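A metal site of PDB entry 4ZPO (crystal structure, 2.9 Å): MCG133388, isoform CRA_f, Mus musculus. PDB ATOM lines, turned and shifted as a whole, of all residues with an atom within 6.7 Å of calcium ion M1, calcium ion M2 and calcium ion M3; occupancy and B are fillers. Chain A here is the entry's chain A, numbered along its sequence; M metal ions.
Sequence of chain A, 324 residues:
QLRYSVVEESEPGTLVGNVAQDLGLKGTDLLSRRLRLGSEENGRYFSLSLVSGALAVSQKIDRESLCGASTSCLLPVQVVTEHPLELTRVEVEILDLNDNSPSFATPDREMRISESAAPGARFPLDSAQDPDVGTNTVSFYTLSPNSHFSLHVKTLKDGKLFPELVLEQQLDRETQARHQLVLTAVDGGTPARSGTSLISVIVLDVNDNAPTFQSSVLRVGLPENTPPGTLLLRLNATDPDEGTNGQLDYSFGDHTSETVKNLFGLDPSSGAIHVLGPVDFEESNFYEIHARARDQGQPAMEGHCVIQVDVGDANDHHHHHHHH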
ATOM      1  N   GLU A 115     -11.183  -8.527  14.294  1.00  0.00           N
ATOM      2  CA  GLU A 115     -11.310  -7.079  14.238  1.00  0.00           C
ATOM      3  C   GLU A 115     -10.563  -6.424  15.404  1.00  0.00           C
ATOM      4  O   GLU A 115     -10.253  -5.233  15.362  1.00  0.00           O
ATOM      5  CB  GLU A 115     -12.781  -6.675  14.257  1.00  0.00           C
ATOM      6  CG  GLU A 115     -13.060  -5.226  13.926  1.00  0.00           C
ATOM      7  CD  GLU A 115     -14.538  -4.912  13.954  1.00  0.00           C
ATOM      8  OE1 GLU A 115     -15.335  -5.815  14.270  1.00  0.00           O
ATOM      9  OE2 GLU A 115     -14.899  -3.751  13.660  1.00  0.00           O
ATOM     10  N   GLN A 170      -5.682  -0.215  13.059  1.00  0.00           N
ATOM     11  CA  GLN A 170      -6.704  -1.158  13.508  1.00  0.00           C
ATOM     12  C   GLN A 170      -7.764  -1.398  12.437  1.00  0.00           C
ATOM     13  O   GLN A 170      -8.287  -0.451  11.847  1.00  0.00           O
ATOM     14  CB  GLN A 170      -7.360  -0.660  14.788  1.00  0.00           C
ATOM     15  CG  GLN A 170      -8.482  -1.549  15.306  1.00  0.00           C
ATOM     16  CD  GLN A 170      -8.018  -2.966  15.595  1.00  0.00           C
ATOM     17  OE1 GLN A 170      -7.962  -3.808  14.694  1.00  0.00           O
ATOM     18  NE2 GLN A 170      -7.684  -3.238  16.848  1.00  0.00           N
ATOM     19  N   LEU A 171      -8.083  -2.663  12.207  1.00  0.00           N
ATOM     20  CA  LEU A 171      -9.103  -3.028  11.229  1.00  0.00           C
ATOM     21  C   LEU A 171     -10.499  -2.732  11.772  1.00  0.00           C
ATOM     22  O   LEU A 171     -10.717  -2.733  12.982  1.00  0.00           O
ATOM     23  CB  LEU A 171      -8.991  -4.515  10.873  1.00  0.00           C
ATOM     24  CG  LEU A 171      -7.636  -4.994  10.351  1.00  0.00           C
ATOM     25  CD1 LEU A 171      -7.649  -6.494  10.132  1.00  0.00           C
ATOM     26  CD2 LEU A 171      -7.263  -4.261   9.074  1.00  0.00           C
ATOM     27  N   ASP A 172     -11.438  -2.473  10.869  1.00  0.00           N
ATOM     28  CA  ASP A 172     -12.812  -2.191  11.256  1.00  0.00           C
ATOM     29  C   ASP A 172     -13.786  -2.826  10.274  1.00  0.00           C
ATOM     30  O   ASP A 172     -13.952  -2.357   9.146  1.00  0.00           O
ATOM     31  CB  ASP A 172     -13.048  -0.686  11.335  1.00  0.00           C
ATOM     32  CG  ASP A 172     -14.435  -0.332  11.833  1.00  0.00           C
ATOM     33  OD1 ASP A 172     -15.046  -1.157  12.531  1.00  0.00           O
ATOM     34  OD2 ASP A 172     -14.919   0.787  11.525  1.00  0.00           O
ATOM     35  N   ARG A 173     -14.449  -3.898  10.715  1.00  0.00           N
ATOM     36  CA  ARG A 173     -15.376  -4.643   9.871  1.00  0.00           C
ATOM     37  C   ARG A 173     -16.552  -3.790   9.419  1.00  0.00           C
ATOM     38  O   ARG A 173     -17.129  -4.007   8.355  1.00  0.00           O
ATOM     39  CB  ARG A 173     -15.892  -5.883  10.618  1.00  0.00           C
ATOM     40  CG  ARG A 173     -16.800  -6.760   9.789  1.00  0.00           C
ATOM     41  CD  ARG A 173     -17.685  -7.624  10.665  1.00  0.00           C
ATOM     42  NE  ARG A 173     -18.995  -7.836  10.048  1.00  0.00           N
ATOM     43  CZ  ARG A 173     -20.028  -7.024  10.205  1.00  0.00           C
ATOM     44  NH1 ARG A 173     -19.916  -5.942  10.965  1.00  0.00           N
ATOM     45  NH2 ARG A 173     -21.180  -7.283   9.602  1.00  0.00           N
ATOM     46  N   GLU A 174     -16.910  -2.789  10.225  1.00  0.00           N
ATOM     47  CA  GLU A 174     -18.039  -1.917   9.917  1.00  0.00           C
ATOM     48  C   GLU A 174     -17.772  -1.024   8.707  1.00  0.00           C
ATOM     49  O   GLU A 174     -18.703  -0.503   8.101  1.00  0.00           O
ATOM     50  CB  GLU A 174     -18.406  -1.066  11.131  1.00  0.00           C
ATOM     51  CG  GLU A 174     -19.263  -1.786  12.171  1.00  0.00           C
ATOM     52  CD  GLU A 174     -18.504  -2.843  12.943  1.00  0.00           C
ATOM     53  OE1 GLU A 174     -18.984  -3.987  13.019  1.00  0.00           O
ATOM     54  OE2 GLU A 174     -17.426  -2.524  13.479  1.00  0.00           O
ATOM     55  N   LEU A 204     -12.864 -10.740  10.814  1.00  0.00           N
ATOM     56  CA  LEU A 204     -13.869 -11.377  11.667  1.00  0.00           C
ATOM     57  C   LEU A 204     -14.484 -10.353  12.609  1.00  0.00           C
ATOM     58  O   LEU A 204     -13.813  -9.408  13.031  1.00  0.00           O
ATOM     59  CB  LEU A 204     -13.236 -12.520  12.467  1.00  0.00           C
ATOM     60  CG  LEU A 204     -12.642 -13.659  11.646  1.00  0.00           C
ATOM     61  CD1 LEU A 204     -11.998 -14.714  12.538  1.00  0.00           C
ATOM     62  CD2 LEU A 204     -13.701 -14.290  10.749  1.00  0.00           C
ATOM     63  N   ASP A 205     -15.753 -10.532  12.932  1.00  0.00           N
ATOM     64  CA  ASP A 205     -16.487  -9.550  13.723  1.00  0.00           C
ATOM     65  C   ASP A 205     -16.140  -9.592  15.208  1.00  0.00           C
ATOM     66  O   ASP A 205     -15.934 -10.665  15.788  1.00  0.00           O
ATOM     67  CB  ASP A 205     -17.989  -9.738  13.556  1.00  0.00           C
ATOM     68  CG  ASP A 205     -18.795  -8.620  14.198  1.00  0.00           C
ATOM     69  OD1 ASP A 205     -18.380  -7.453  14.088  1.00  0.00           O
ATOM     70  OD2 ASP A 205     -19.841  -8.923  14.825  1.00  0.00           O
ATOM     71  N   VAL A 206     -16.070  -8.413  15.813  1.00  0.00           N
ATOM     72  CA  VAL A 206     -15.894  -8.275  17.254  1.00  0.00           C
ATOM     73  C   VAL A 206     -16.901  -7.239  17.754  1.00  0.00           C
ATOM     74  O   VAL A 206     -17.117  -6.227  17.095  1.00  0.00           O
ATOM     75  CB  VAL A 206     -14.458  -7.835  17.622  1.00  0.00           C
ATOM     76  CG1 VAL A 206     -14.365  -7.451  19.095  1.00  0.00           C
ATOM     77  CG2 VAL A 206     -13.460  -8.924  17.292  1.00  0.00           C
ATOM     78  N   ASN A 207     -17.539  -7.513  18.892  1.00  0.00           N
ATOM     79  CA  ASN A 207     -18.508  -6.570  19.446  1.00  0.00           C
ATOM     80  C   ASN A 207     -17.823  -5.272  19.874  1.00  0.00           C
ATOM     81  O   ASN A 207     -17.498  -5.096  21.047  1.00  0.00           O
ATOM     82  CB  ASN A 207     -19.253  -7.192  20.624  1.00  0.00           C
ATOM     83  CG  ASN A 207     -20.554  -6.466  20.935  1.00  0.00           C
ATOM     84  OD1 ASN A 207     -20.681  -5.262  20.718  1.00  0.00           O
ATOM     85  ND2 ASN A 207     -21.530  -7.195  21.440  1.00  0.00           N
ATOM     86  N   ASP A 208     -17.610  -4.375  18.921  1.00  0.00           N
ATOM     87  CA  ASP A 208     -16.972  -3.096  19.206  1.00  0.00           C
ATOM     88  C   ASP A 208     -17.932  -1.934  18.945  1.00  0.00           C
ATOM     89  O   ASP A 208     -17.508  -0.815  18.675  1.00  0.00           O
ATOM     90  CB  ASP A 208     -15.705  -2.930  18.358  1.00  0.00           C
ATOM     91  CG  ASP A 208     -16.001  -2.792  16.874  1.00  0.00           C
ATOM     92  OD1 ASP A 208     -16.192  -3.825  16.204  1.00  0.00           O
ATOM     93  OD2 ASP A 208     -16.037  -1.644  16.378  1.00  0.00           O
ATOM     94  N   ASN A 209     -19.225  -2.222  19.022  1.00  0.00           N
ATOM     95  CA  ASN A 209     -20.245  -1.194  18.856  1.00  0.00           C
ATOM     96  C   ASN A 209     -21.394  -1.360  19.837  1.00  0.00           C
ATOM     97  O   ASN A 209     -21.805  -2.486  20.141  1.00  0.00           O
ATOM     98  CB  ASN A 209     -20.773  -1.197  17.427  1.00  0.00           C
ATOM     99  CG  ASN A 209     -19.870  -0.443  16.457  1.00  0.00           C
ATOM    100  OD1 ASN A 209     -18.914  -1.008  15.928  1.00  0.00           O
ATOM    101  ND2 ASN A 209     -20.181   0.823  16.234  1.00  0.00           N
ATOM    102  N   ALA A 210     -21.894  -0.241  20.343  1.00  0.00           N
ATOM    103  CA  ALA A 210     -23.031  -0.255  21.247  1.00  0.00           C
ATOM    104  C   ALA A 210     -24.282   0.205  20.522  1.00  0.00           C
ATOM    105  O   ALA A 210     -24.206   1.061  19.634  1.00  0.00           O
ATOM    106  CB  ALA A 210     -22.764   0.611  22.467  1.00  0.00           C
ATOM    107  N   PRO A 211     -25.447  -0.357  20.882  1.00  0.00           N
ATOM    108  CA  PRO A 211     -26.721   0.074  20.296  1.00  0.00           C
ATOM    109  C   PRO A 211     -26.948   1.571  20.499  1.00  0.00           C
ATOM    110  O   PRO A 211     -26.551   2.110  21.524  1.00  0.00           O
ATOM    111  CB  PRO A 211     -27.759  -0.752  21.057  1.00  0.00           C
ATOM    112  CG  PRO A 211     -27.015  -1.963  21.499  1.00  0.00           C
ATOM    113  CD  PRO A 211     -25.627  -1.489  21.811  1.00  0.00           C
ATOM    114  N   ASP A 239     -27.643  -1.337  15.546  1.00  0.00           N
ATOM    115  CA  ASP A 239     -26.352  -1.891  15.904  1.00  0.00           C
ATOM    116  C   ASP A 239     -25.684  -2.474  14.664  1.00  0.00           C
ATOM    117  O   ASP A 239     -26.191  -3.430  14.068  1.00  0.00           O
ATOM    118  CB  ASP A 239     -26.501  -2.955  16.989  1.00  0.00           C
ATOM    119  CG  ASP A 239     -25.194  -3.266  17.682  1.00  0.00           C
ATOM    120  OD1 ASP A 239     -24.356  -3.974  17.088  1.00  0.00           O
ATOM    121  OD2 ASP A 239     -24.994  -2.792  18.822  1.00  0.00           O
ATOM    122  N   PRO A 240     -24.542  -1.903  14.259  1.00  0.00           N
ATOM    123  CA  PRO A 240     -23.847  -2.253  13.011  1.00  0.00           C
ATOM    124  C   PRO A 240     -23.092  -3.586  13.078  1.00  0.00           C
ATOM    125  O   PRO A 240     -22.602  -4.047  12.047  1.00  0.00           O
ATOM    126  CB  PRO A 240     -22.886  -1.089  12.819  1.00  0.00           C
ATOM    127  CG  PRO A 240     -22.568  -0.639  14.202  1.00  0.00           C
ATOM    128  CD  PRO A 240     -23.844  -0.829  14.996  1.00  0.00           C
ATOM    129  N   ASP A 241     -22.981  -4.168  14.261  1.00  0.00           N
ATOM    130  CA  ASP A 241     -22.220  -5.410  14.426  1.00  0.00           C
ATOM    131  C   ASP A 241     -22.953  -6.599  13.813  1.00  0.00           C
ATOM    132  O   ASP A 241     -24.151  -6.546  13.546  1.00  0.00           O
ATOM    133  CB  ASP A 241     -21.933  -5.665  15.904  1.00  0.00           C
ATOM    134  CG  ASP A 241     -20.955  -4.669  16.484  1.00  0.00           C
ATOM    135  OD1 ASP A 241     -20.170  -4.078  15.713  1.00  0.00           O
ATOM    136  OD2 ASP A 241     -20.950  -4.480  17.723  1.00  0.00           O
ATOM    137  N   GLU A 242     -22.203  -7.677  13.589  1.00  0.00           N
ATOM    138  CA  GLU A 242     -22.715  -8.854  12.888  1.00  0.00           C
ATOM    139  C   GLU A 242     -23.310  -9.894  13.828  1.00  0.00           C
ATOM    140  O   GLU A 242     -22.791 -10.128  14.926  1.00  0.00           O
ATOM    141  CB  GLU A 242     -21.593  -9.492  12.057  1.00  0.00           C
ATOM    142  CG  GLU A 242     -22.011 -10.693  11.232  1.00  0.00           C
ATOM    143  CD  GLU A 242     -20.857 -11.299  10.473  1.00  0.00           C
ATOM    144  OE1 GLU A 242     -19.711 -10.832  10.645  1.00  0.00           O
ATOM    145  OE2 GLU A 242     -21.087 -12.258   9.698  1.00  0.00           O
ATOM    146  N   THR A 244     -25.355 -12.003  16.493  1.00  0.00           N
ATOM    147  CA  THR A 244     -25.877 -11.737  17.830  1.00  0.00           C
ATOM    148  C   THR A 244     -25.303 -10.443  18.402  1.00  0.00           C
ATOM    149  O   THR A 244     -25.915  -9.813  19.259  1.00  0.00           O
ATOM    150  CB  THR A 244     -25.566 -12.899  18.796  1.00  0.00           C
ATOM    151  OG1 THR A 244     -24.146 -13.070  18.893  1.00  0.00           O
ATOM    152  CG2 THR A 244     -26.200 -14.181  18.297  1.00  0.00           C
ATOM    153  N   ASN A 245     -24.136 -10.054  17.913  1.00  0.00           N
ATOM    154  CA  ASN A 245     -23.516  -8.802  18.323  1.00  0.00           C
ATOM    155  C   ASN A 245     -24.300  -7.602  17.819  1.00  0.00           C
ATOM    156  O   ASN A 245     -24.131  -6.486  18.316  1.00  0.00           O
ATOM    157  CB  ASN A 245     -22.069  -8.736  17.831  1.00  0.00           C
ATOM    158  CG  ASN A 245     -21.159  -9.733  18.509  1.00  0.00           C
ATOM    159  OD1 ASN A 245     -21.629 -10.650  19.190  1.00  0.00           O
ATOM    160  ND2 ASN A 245     -19.854  -9.577  18.331  1.00  0.00           N
ATOM    161  N   GLY A 246     -25.164  -7.826  16.836  1.00  0.00           N
ATOM    162  CA  GLY A 246     -25.967  -6.770  16.255  1.00  0.00           C
ATOM    163  C   GLY A 246     -27.409  -6.765  16.718  1.00  0.00           C
ATOM    164  O   GLY A 246     -28.097  -5.755  16.627  1.00  0.00           O
ATOM    165  N   GLN A 247     -27.877  -7.908  17.213  1.00  0.00           N
ATOM    166  CA  GLN A 247     -29.239  -8.018  17.725  1.00  0.00           C
ATOM    167  C   GLN A 247     -29.327  -7.444  19.138  1.00  0.00           C
ATOM    168  O   GLN A 247     -28.378  -7.552  19.918  1.00  0.00           O
ATOM    169  CB  GLN A 247     -29.716  -9.472  17.704  1.00  0.00           C
ATOM    170  CG  GLN A 247     -29.996 -10.000  16.302  1.00  0.00           C
ATOM    171  CD  GLN A 247     -30.586 -11.394  16.315  1.00  0.00           C
ATOM    172  OE1 GLN A 247     -30.039 -12.316  16.926  1.00  0.00           O
ATOM    173  NE2 GLN A 247     -31.721 -11.556  15.647  1.00  0.00           N
ATOM    174  N   ASP A 295     -27.358  -5.235  24.189  1.00  0.00           N
ATOM    175  CA  ASP A 295     -26.791  -6.072  23.134  1.00  0.00           C
ATOM    176  C   ASP A 295     -26.877  -7.540  23.508  1.00  0.00           C
ATOM    177  O   ASP A 295     -27.269  -7.886  24.626  1.00  0.00           O
ATOM    178  CB  ASP A 295     -25.339  -5.680  22.861  1.00  0.00           C
ATOM    179  CG  ASP A 295     -24.929  -5.930  21.434  1.00  0.00           C
ATOM    180  OD1 ASP A 295     -25.690  -6.575  20.701  1.00  0.00           O
ATOM    181  OD2 ASP A 295     -23.816  -5.490  21.059  1.00  0.00           O
ATOM    182  N   GLN A 296     -26.515  -8.420  22.578  1.00  0.00           N
ATOM    183  CA  GLN A 296     -26.515  -9.857  22.844  1.00  0.00           C
ATOM    184  C   GLN A 296     -25.126 -10.459  22.659  1.00  0.00           C
ATOM    185  O   GLN A 296     -24.969 -11.683  22.607  1.00  0.00           O
ATOM    186  CB  GLN A 296     -27.514 -10.567  21.936  1.00  0.00           C
ATOM    187  CG  GLN A 296     -28.965 -10.279  22.259  1.00  0.00           C
ATOM    188  CD  GLN A 296     -29.921 -11.163  21.481  1.00  0.00           C
ATOM    189  OE1 GLN A 296     -29.505 -12.062  20.757  1.00  0.00           O
ATOM    190  NE2 GLN A 296     -31.220 -10.912  21.635  1.00  0.00           N
ATOM    191  N   GLY A 297     -24.119  -9.604  22.568  1.00  0.00           N
ATOM    192  CA  GLY A 297     -22.749 -10.064  22.408  1.00  0.00           C
ATOM    193  C   GLY A 297     -22.034 -10.218  23.738  1.00  0.00           C
ATOM    194  O   GLY A 297     -22.576  -9.904  24.788  1.00  0.00           O
ATOM    195  N   MET A 301     -23.081  -4.766  25.095  1.00  0.00           N
ATOM    196  CA  MET A 301     -23.081  -3.309  24.986  1.00  0.00           C
ATOM    197  C   MET A 301     -24.504  -2.782  25.157  1.00  0.00           C
ATOM    198  O   MET A 301     -25.467  -3.549  25.092  1.00  0.00           O
ATOM    199  CB  MET A 301     -22.515  -2.874  23.635  1.00  0.00           C
ATOM    200  CG  MET A 301     -21.109  -3.381  23.339  1.00  0.00           C
ATOM    201  SD  MET A 301     -19.872  -2.758  24.497  1.00  0.00           S
ATOM    202  CE  MET A 301     -18.371  -3.061  23.575  1.00  0.00           C
HETATM  203 CA    CA M   1     -17.854  -5.181  14.942  1.00  0.00          CA
HETATM  204 CA    CA M   2     -22.969  -4.369  19.123  1.00  0.00          CA
HETATM  205 CA    CA M   3     -14.187  -1.662  14.793  1.00  0.00          CA
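ND2 of Asn 207 lies close to OD2 of Asp 295, 2.9 Å away. O of Met 301 sits at hydrogen-bond distance from N of Asp 295. OD1 of Asn 209 sits close to OD2 of Asp 208, at 3.0 Å. The side-chain amide oxygen (OD1) of Asn 209 sits close to the side-chain carboxylate (OE2) of Glu 174 (3.2 Å). The backbone NH of Arg 173 sits close to the side-chain carboxylate of Glu 115. The backbone NH of Glu 115 is in hydrogen-bond range of the backbone carbonyl oxygen of Leu 204. NH1 of Arg 173 sits close to OE1 of Glu 174 (3.0 Å). ND2 of Asn 245 lies close to N of Asn 207, at 3.2 Å.
Of the 26 residues printed, 6 come within 4 Å of calcium ion M1.
Along chain A the residues within 4 Å of calcium ion M2 span positions 207 to 295.
Four residues have an atom within 4 Å of calcium ion M3: Glu 115, Asp 172, Glu 174 and Asp 208. The nearest printed residue that does not touch calcium ion M3 is Leu 171 (4.1 Å).
Calcium ion M1 is bound by OD1 of Asp 205 (2.5 Å). OD1 of Asp 208 is bound to calcium ion M1, at 2.5 Å. Calcium ion M1 is bound by the backbone carbonyl oxygen (O) of Val 206 (2.5 Å). Calcium ion M1 is bound by OE1 of Glu 174 (2.5 Å). Calcium ion M1 is bound by the side-chain carboxylate (OD1) of Asp 241 (2.7 Å). The side-chain carboxylate (OE1) of Glu 115 binds calcium ion M1, 2.7 Å away. Slightly farther from calcium ion M1 lies OE2 of Glu 174 (3.1 Å).
Calcium ion M2 is bound by the side-chain carboxylate (OD2) of Asp 295 (2.4 Å), the backbone carbonyl oxygen (O) of Asn 209 (2.4 Å), the side-chain carboxylate (OD2) of Asp 241 (2.5 Å), the side-chain carboxylate (OD1) of Asp 239 (2.5 Å), the backbone carbonyl oxygen (O) of Asn 245 (2.5 Å) and the side-chain carboxylate (OD2) of Asp 239 (2.6 Å). Calcium ion M2 has six donor atoms within binding distance. Slightly farther from calcium ion M2 lies the side-chain amide oxygen (OD1) of Asn 207 (2.9 Å).
Calcium ion M3 is bound by the side-chain carboxylate (OD2) of Asp 208 (2.4 Å), the side-chain carboxylate (OD1) of Asp 172 (2.5 Å) and the side-chain carboxylate (OE2) of Glu 115 (2.5 Å). Calcium ion M3 has three donor atoms within binding distance.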
